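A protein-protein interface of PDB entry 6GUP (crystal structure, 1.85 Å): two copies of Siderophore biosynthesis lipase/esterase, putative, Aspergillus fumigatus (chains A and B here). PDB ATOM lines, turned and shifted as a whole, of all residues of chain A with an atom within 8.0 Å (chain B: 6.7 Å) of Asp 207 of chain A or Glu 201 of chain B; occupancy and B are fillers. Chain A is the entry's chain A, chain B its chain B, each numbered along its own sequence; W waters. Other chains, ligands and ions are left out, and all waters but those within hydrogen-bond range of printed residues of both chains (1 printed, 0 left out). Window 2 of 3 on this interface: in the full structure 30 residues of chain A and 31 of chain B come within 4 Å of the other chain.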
ATOM      1  N   ALA A 202     -21.551   0.571  10.633  1.00  0.00           N
ATOM      2  CA  ALA A 202     -20.693   0.989  11.747  1.00  0.00           C
ATOM      3  C   ALA A 202     -19.630   2.005  11.325  1.00  0.00           C
ATOM      4  O   ALA A 202     -19.353   2.948  12.065  1.00  0.00           O
ATOM      5  CB  ALA A 202     -20.033  -0.220  12.388  1.00  0.00           C
ATOM      6  N   ALA A 203     -19.041   1.815  10.145  1.00  0.00           N
ATOM      7  CA  ALA A 203     -18.055   2.761   9.605  1.00  0.00           C
ATOM      8  C   ALA A 203     -18.652   4.159   9.423  1.00  0.00           C
ATOM      9  O   ALA A 203     -18.018   5.160   9.759  1.00  0.00           O
ATOM     10  CB  ALA A 203     -17.490   2.252   8.287  1.00  0.00           C
ATOM     11  N   ARG A 204     -19.877   4.212   8.903  1.00  0.00           N
ATOM     12  CA  ARG A 204     -20.605   5.472   8.741  1.00  0.00           C
ATOM     13  C   ARG A 204     -21.074   6.085  10.068  1.00  0.00           C
ATOM     14  O   ARG A 204     -20.919   7.292  10.276  1.00  0.00           O
ATOM     15  CB  ARG A 204     -21.826   5.275   7.837  1.00  0.00           C
ATOM     16  CG  ARG A 204     -21.507   4.970   6.381  1.00  0.00           C
ATOM     17  CD  ARG A 204     -22.767   5.060   5.532  1.00  0.00           C
ATOM     18  NE  ARG A 204     -23.774   4.076   5.942  1.00  0.00           N
ATOM     19  CZ  ARG A 204     -23.941   2.856   5.421  1.00  0.00           C
ATOM     20  NH1 ARG A 204     -23.175   2.403   4.426  1.00  0.00           N
ATOM     21  NH2 ARG A 204     -24.900   2.069   5.903  1.00  0.00           N
ATOM     22  N   ASP A 205     -21.636   5.255  10.951  1.00  0.00           N
ATOM     23  CA  ASP A 205     -22.429   5.731  12.100  1.00  0.00           C
ATOM     24  C   ASP A 205     -21.751   5.714  13.476  1.00  0.00           C
ATOM     25  O   ASP A 205     -22.198   6.431  14.373  1.00  0.00           O
ATOM     26  CB  ASP A 205     -23.738   4.930  12.192  1.00  0.00           C
ATOM     27  CG  ASP A 205     -24.621   5.083  10.954  1.00  0.00           C
ATOM     28  OD1 ASP A 205     -24.276   5.863  10.039  1.00  0.00           O
ATOM     29  OD2 ASP A 205     -25.676   4.419  10.898  1.00  0.00           O
ATOM     30  N   ALA A 206     -20.706   4.905  13.662  1.00  0.00           N
ATOM     31  CA  ALA A 206     -20.057   4.788  14.978  1.00  0.00           C
ATOM     32  C   ALA A 206     -19.321   6.072  15.351  1.00  0.00           C
ATOM     33  O   ALA A 206     -18.795   6.767  14.477  1.00  0.00           O
ATOM     34  CB  ALA A 206     -19.099   3.606  15.012  1.00  0.00           C
ATOM     35  N   ASP A 207     -19.295   6.383  16.647  1.00  0.00           N
ATOM     36  CA  ASP A 207     -18.585   7.563  17.152  1.00  0.00           C
ATOM     37  C   ASP A 207     -17.083   7.412  16.939  1.00  0.00           C
ATOM     38  O   ASP A 207     -16.564   6.295  16.912  1.00  0.00           O
ATOM     39  CB  ASP A 207     -18.874   7.792  18.644  1.00  0.00           C
ATOM     40  CG  ASP A 207     -20.307   8.228  18.909  1.00  0.00           C
ATOM     41  OD1 ASP A 207     -20.804   9.140  18.213  1.00  0.00           O
ATOM     42  OD2 ASP A 207     -20.934   7.666  19.831  1.00  0.00           O
ATOM     43  N   ALA A 208     -16.395   8.540  16.777  1.00  0.00           N
ATOM     44  CA  ALA A 208     -14.948   8.539  16.570  1.00  0.00           C
ATOM     45  C   ALA A 208     -14.235   7.916  17.769  1.00  0.00           C
ATOM     46  O   ALA A 208     -14.597   8.183  18.917  1.00  0.00           O
ATOM     47  CB  ALA A 208     -14.441   9.949  16.330  1.00  0.00           C
ATOM     48  N   GLY A 209     -13.255   7.060  17.489  1.00  0.00           N
ATOM     49  CA  GLY A 209     -12.511   6.349  18.529  1.00  0.00           C
ATOM     50  C   GLY A 209     -13.118   5.038  19.011  1.00  0.00           C
ATOM     51  O   GLY A 209     -12.435   4.270  19.691  1.00  0.00           O
ATOM     52  N   THR A 210     -14.386   4.774  18.678  1.00  0.00           N
ATOM     53  CA  THR A 210     -15.042   3.521  19.062  1.00  0.00           C
ATOM     54  C   THR A 210     -14.790   2.427  18.032  1.00  0.00           C
ATOM     55  O   THR A 210     -14.443   2.707  16.880  1.00  0.00           O
ATOM     56  CB  THR A 210     -16.572   3.672  19.227  1.00  0.00           C
ATOM     57  OG1 THR A 210     -17.171   4.025  17.975  1.00  0.00           O
ATOM     58  CG2 THR A 210     -16.907   4.727  20.255  1.00  0.00           C
ATOM     59  N   ASP A 211     -14.977   1.183  18.467  1.00  0.00           N
ATOM     60  CA  ASP A 211     -14.908   0.010  17.600  1.00  0.00           C
ATOM     61  C   ASP A 211     -16.120  -0.874  17.858  1.00  0.00           C
ATOM     62  O   ASP A 211     -16.321  -1.338  18.982  1.00  0.00           O
ATOM     63  CB  ASP A 211     -13.627  -0.788  17.868  1.00  0.00           C
ATOM     64  CG  ASP A 211     -12.449  -0.289  17.061  1.00  0.00           C
ATOM     65  OD1 ASP A 211     -12.502  -0.364  15.814  1.00  0.00           O
ATOM     66  OD2 ASP A 211     -11.464   0.176  17.669  1.00  0.00           O
ATOM     67  N   VAL A 212     -16.921  -1.099  16.818  1.00  0.00           N
ATOM     68  CA  VAL A 212     -18.054  -2.014  16.889  1.00  0.00           C
ATOM     69  C   VAL A 212     -17.532  -3.418  16.602  1.00  0.00           C
ATOM     70  O   VAL A 212     -17.185  -3.733  15.463  1.00  0.00           O
ATOM     71  CB  VAL A 212     -19.165  -1.634  15.882  1.00  0.00           C
ATOM     72  CG1 VAL A 212     -20.339  -2.604  15.976  1.00  0.00           C
ATOM     73  CG2 VAL A 212     -19.640  -0.208  16.130  1.00  0.00           C
ATOM     74  N   ARG A 232     -14.443  -2.026  11.407  1.00  0.00           N
ATOM     75  CA  ARG A 232     -13.401  -1.407  10.582  1.00  0.00           C
ATOM     76  C   ARG A 232     -12.387  -2.416  10.060  1.00  0.00           C
ATOM     77  O   ARG A 232     -11.963  -2.321   8.905  1.00  0.00           O
ATOM     78  CB  ARG A 232     -12.673  -0.299  11.345  1.00  0.00           C
ATOM     79  CG  ARG A 232     -13.494   0.970  11.469  1.00  0.00           C
ATOM     80  CD  ARG A 232     -12.679   2.107  12.053  1.00  0.00           C
ATOM     81  NE  ARG A 232     -12.325   1.889  13.453  1.00  0.00           N
ATOM     82  CZ  ARG A 232     -11.694   2.778  14.223  1.00  0.00           C
ATOM     83  NH1 ARG A 232     -11.338   3.971  13.747  1.00  0.00           N
ATOM     84  NH2 ARG A 232     -11.418   2.479  15.486  1.00  0.00           N
ATOM     85  N   LYS B 194     -18.061  12.826  28.371  1.00  0.00           N
ATOM     86  CA  LYS B 194     -18.039  12.441  26.958  1.00  0.00           C
ATOM     87  C   LYS B 194     -18.176  10.927  26.811  1.00  0.00           C
ATOM     88  O   LYS B 194     -18.963  10.463  25.991  1.00  0.00           O
ATOM     89  CB  LYS B 194     -16.765  12.942  26.263  1.00  0.00           C
ATOM     90  CG  LYS B 194     -16.684  12.657  24.766  1.00  0.00           C
ATOM     91  CD  LYS B 194     -17.783  13.349  23.968  1.00  0.00           C
ATOM     92  CE  LYS B 194     -17.693  13.024  22.485  1.00  0.00           C
ATOM     93  NZ  LYS B 194     -16.478  13.592  21.840  1.00  0.00           N
ATOM     94  N   THR B 196     -19.600   8.947  28.924  1.00  0.00           N
ATOM     95  CA  THR B 196     -21.007   8.708  29.247  1.00  0.00           C
ATOM     96  C   THR B 196     -21.872   8.928  28.001  1.00  0.00           C
ATOM     97  O   THR B 196     -22.659   8.057  27.635  1.00  0.00           O
ATOM     98  CB  THR B 196     -21.487   9.620  30.400  1.00  0.00           C
ATOM     99  OG1 THR B 196     -20.636   9.439  31.539  1.00  0.00           O
ATOM    100  CG2 THR B 196     -22.929   9.313  30.793  1.00  0.00           C
ATOM    101  N   SER B 197     -21.695  10.079  27.351  1.00  0.00           N
ATOM    102  CA  SER B 197     -22.424  10.418  26.117  1.00  0.00           C
ATOM    103  C   SER B 197     -22.140   9.443  24.965  1.00  0.00           C
ATOM    104  O   SER B 197     -23.050   9.096  24.207  1.00  0.00           O
ATOM    105  CB  SER B 197     -22.100  11.853  25.682  1.00  0.00           C
ATOM    106  OG  SER B 197     -22.786  12.204  24.490  1.00  0.00           O
ATOM    107  N   MET B 198     -20.883   9.020  24.839  1.00  0.00           N
ATOM    108  CA  MET B 198     -20.489   8.002  23.858  1.00  0.00           C
ATOM    109  C   MET B 198     -21.095   6.631  24.176  1.00  0.00           C
ATOM    110  O   MET B 198     -21.505   5.909  23.266  1.00  0.00           O
ATOM    111  CB  MET B 198     -18.961   7.883  23.781  1.00  0.00           C
ATOM    112  CG  MET B 198     -18.276   9.095  23.165  1.00  0.00           C
ATOM    113  SD  MET B 198     -16.493   8.901  23.018  1.00  0.00           S
ATOM    114  CE  MET B 198     -16.425   7.657  21.738  1.00  0.00           C
ATOM    115  N   ALA B 199     -21.150   6.287  25.464  1.00  0.00           N
ATOM    116  CA  ALA B 199     -21.667   4.988  25.908  1.00  0.00           C
ATOM    117  C   ALA B 199     -23.187   4.853  25.783  1.00  0.00           C
ATOM    118  O   ALA B 199     -23.675   3.798  25.377  1.00  0.00           O
ATOM    119  CB  ALA B 199     -21.230   4.702  27.337  1.00  0.00           C
ATOM    120  N   ARG B 200     -23.929   5.905  26.135  1.00  0.00           N
ATOM    121  CA  ARG B 200     -25.400   5.896  26.019  1.00  0.00           C
ATOM    122  C   ARG B 200     -25.861   5.766  24.564  1.00  0.00           C
ATOM    123  O   ARG B 200     -26.839   5.071  24.275  1.00  0.00           O
ATOM    124  CB  ARG B 200     -26.022   7.155  26.640  1.00  0.00           C
ATOM    125  CG  ARG B 200     -25.778   7.300  28.137  1.00  0.00           C
ATOM    126  CD  ARG B 200     -26.912   7.999  28.873  1.00  0.00           C
ATOM    127  NE  ARG B 200     -26.915   7.623  30.292  1.00  0.00           N
ATOM    128  CZ  ARG B 200     -26.664   8.423  31.335  1.00  0.00           C
ATOM    129  NH1 ARG B 200     -26.388   9.722  31.195  1.00  0.00           N
ATOM    130  NH2 ARG B 200     -26.703   7.905  32.563  1.00  0.00           N
ATOM    131  N   GLU B 201     -25.149   6.444  23.665  1.00  0.00           N
ATOM    132  CA  GLU B 201     -25.403   6.370  22.222  1.00  0.00           C
ATOM    133  C   GLU B 201     -25.143   4.967  21.655  1.00  0.00           C
ATOM    134  O   GLU B 201     -25.835   4.534  20.731  1.00  0.00           O
ATOM    135  CB  GLU B 201     -24.546   7.409  21.486  1.00  0.00           C
ATOM    136  CG  GLU B 201     -24.901   7.608  20.017  1.00  0.00           C
ATOM    137  CD  GLU B 201     -24.205   8.806  19.386  1.00  0.00           C
ATOM    138  OE1 GLU B 201     -24.528   9.128  18.224  1.00  0.00           O
ATOM    139  OE2 GLU B 201     -23.337   9.428  20.038  1.00  0.00           O
ATOM    140  N   ALA B 202     -24.146   4.271  22.208  1.00  0.00           N
ATOM    141  CA  ALA B 202     -23.859   2.879  21.842  1.00  0.00           C
ATOM    142  C   ALA B 202     -24.959   1.927  22.321  1.00  0.00           C
ATOM    143  O   ALA B 202     -25.439   1.096  21.544  1.00  0.00           O
ATOM    144  CB  ALA B 202     -22.506   2.448  22.393  1.00  0.00           C
ATOM    145  N   ALA B 203     -25.350   2.049  23.590  1.00  0.00           N
ATOM    146  CA  ALA B 203     -26.467   1.268  24.141  1.00  0.00           C
ATOM    147  C   ALA B 203     -27.798   1.917  23.776  1.00  0.00           C
ATOM    148  O   ALA B 203     -28.554   1.387  22.962  1.00  0.00           O
ATOM    149  CB  ALA B 203     -26.346   1.120  25.652  1.00  0.00           C
ATOM    150  N   VAL B 212     -19.732  -2.422  21.647  1.00  0.00           N
ATOM    151  CA  VAL B 212     -19.014  -1.212  21.260  1.00  0.00           C
ATOM    152  C   VAL B 212     -17.912  -0.940  22.274  1.00  0.00           C
ATOM    153  O   VAL B 212     -18.198  -0.732  23.452  1.00  0.00           O
ATOM    154  CB  VAL B 212     -19.964   0.004  21.216  1.00  0.00           C
ATOM    155  CG1 VAL B 212     -19.219   1.269  20.795  1.00  0.00           C
ATOM    156  CG2 VAL B 212     -21.129  -0.270  20.273  1.00  0.00           C
ATOM    157  N   PRO B 215     -13.108   4.513  23.301  1.00  0.00           N
ATOM    158  CA  PRO B 215     -11.703   4.873  23.040  1.00  0.00           C
ATOM    159  C   PRO B 215     -10.796   4.611  24.245  1.00  0.00           C
ATOM    160  O   PRO B 215     -11.078   5.102  25.340  1.00  0.00           O
ATOM    161  CB  PRO B 215     -11.763   6.378  22.734  1.00  0.00           C
ATOM    162  CG  PRO B 215     -13.171   6.657  22.370  1.00  0.00           C
ATOM    163  CD  PRO B 215     -14.022   5.649  23.072  1.00  0.00           C
ATOM    164  N   LEU B 235     -20.914   1.869  31.482  1.00  0.00           N
ATOM    165  CA  LEU B 235     -22.198   2.267  32.074  1.00  0.00           C
ATOM    166  C   LEU B 235     -22.533   1.444  33.314  1.00  0.00           C
ATOM    167  O   LEU B 235     -23.115   1.975  34.256  1.00  0.00           O
ATOM    168  CB  LEU B 235     -23.346   2.166  31.062  1.00  0.00           C
ATOM    169  CG  LEU B 235     -23.359   3.184  29.917  1.00  0.00           C
ATOM    170  CD1 LEU B 235     -24.575   2.949  29.035  1.00  0.00           C
ATOM    171  CD2 LEU B 235     -23.346   4.624  30.412  1.00  0.00           C
HETATM  172  O   HOH W   1     -20.470   5.238  20.878  1.00  0.00           O
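OD2 of Asp 207 of chain A sits close to OE2 of Glu 201 of chain B, at 3.0 Å.
The side-chain hydroxyl (OG1) of Thr 210 of chain A sits at hydrogen-bond distance from the backbone carbonyl oxygen (O) of Asp 207 of chain A, 2.6 Å away. The backbone carbonyl oxygen (O) of Thr 210 of chain A lies within hydrogen-bond range of the guanidinium group (NH2) of Arg 232 of chain A, 3.3 Å away. The side-chain carboxylate of Asp 211 of chain A lies within salt-bridge range of the guanidinium group of Arg 232 of chain A.
Asp 207 of chain A touches Met 198 of chain B. Ala 208 of chain A touches Met 198 of chain B. Gly 209 of chain A touches Pro 215 of chain B. CG2 of Thr 210 of chain A touches CE of Met 198 of chain B, at 3.3 Å. Thr 210 of chain A touches Val 212 of chain B (CB to CG1, 3.9 Å). Asp 211 of chain A touches Val 212 of chain B (O to CA, 3.5 Å).
Asp 207 of chain A touches two residues of chain B. Of the printed residues of chain B, Ala 208 of chain A touches Met 198. Printed residues of chain B within 4 Å of Gly 209 of chain A: Pro 215. Printed residues of chain B within 4 Å of Thr 210 of chain A: Met 198 (3.3 Å) and Val 212 (3.9 Å). Of the printed residues of chain B, Asp 211 of chain A touches Val 212 (3.5 Å). Of the printed residues of chain A, Met 198 of chain B touches Asp 207, Ala 208 and Thr 210. Printed residues of chain A within 4 Å of Glu 201 of chain B: Asp 207 (3.0 Å). No residue of chain A comes within 4 Å of Ala 202 of chain B. The nearest residue of chain B that does not touch Asp 207 of chain A is Ser 197 of chain B (5.1 Å). The nearest printed residue of chain B that does not touch Asp 211 of chain A is Pro 215 of chain B (6.2 Å).
Of the 12 printed residues of chain A, 5 touch a printed residue of chain B. Printed residues of chain A that touch a printed residue of chain B: Asp 207, Ala 208, Gly 209, Thr 210 and Asp 211. Printed residues of chain B that touch a printed residue of chain A: Met 198, Glu 201, Val 212 and Pro 215. Hydrophobic or aromatic side chains of chain B within 4 Å of the printed part of chain A: Met 198, Val 212 and Pro 215. Among the printed residues, 7 pairs touch across the chains. Among the printed residues, no Asp or Glu carboxylate lies within 4 Å of a Lys or Arg side-chain nitrogen of the other chain.
Positions printed for both chains: 202, 203 and 212.
Water W1 lies within hydrogen-bond range of OD2 of Asp 207 of chain A and O of Met 198 of chain B.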
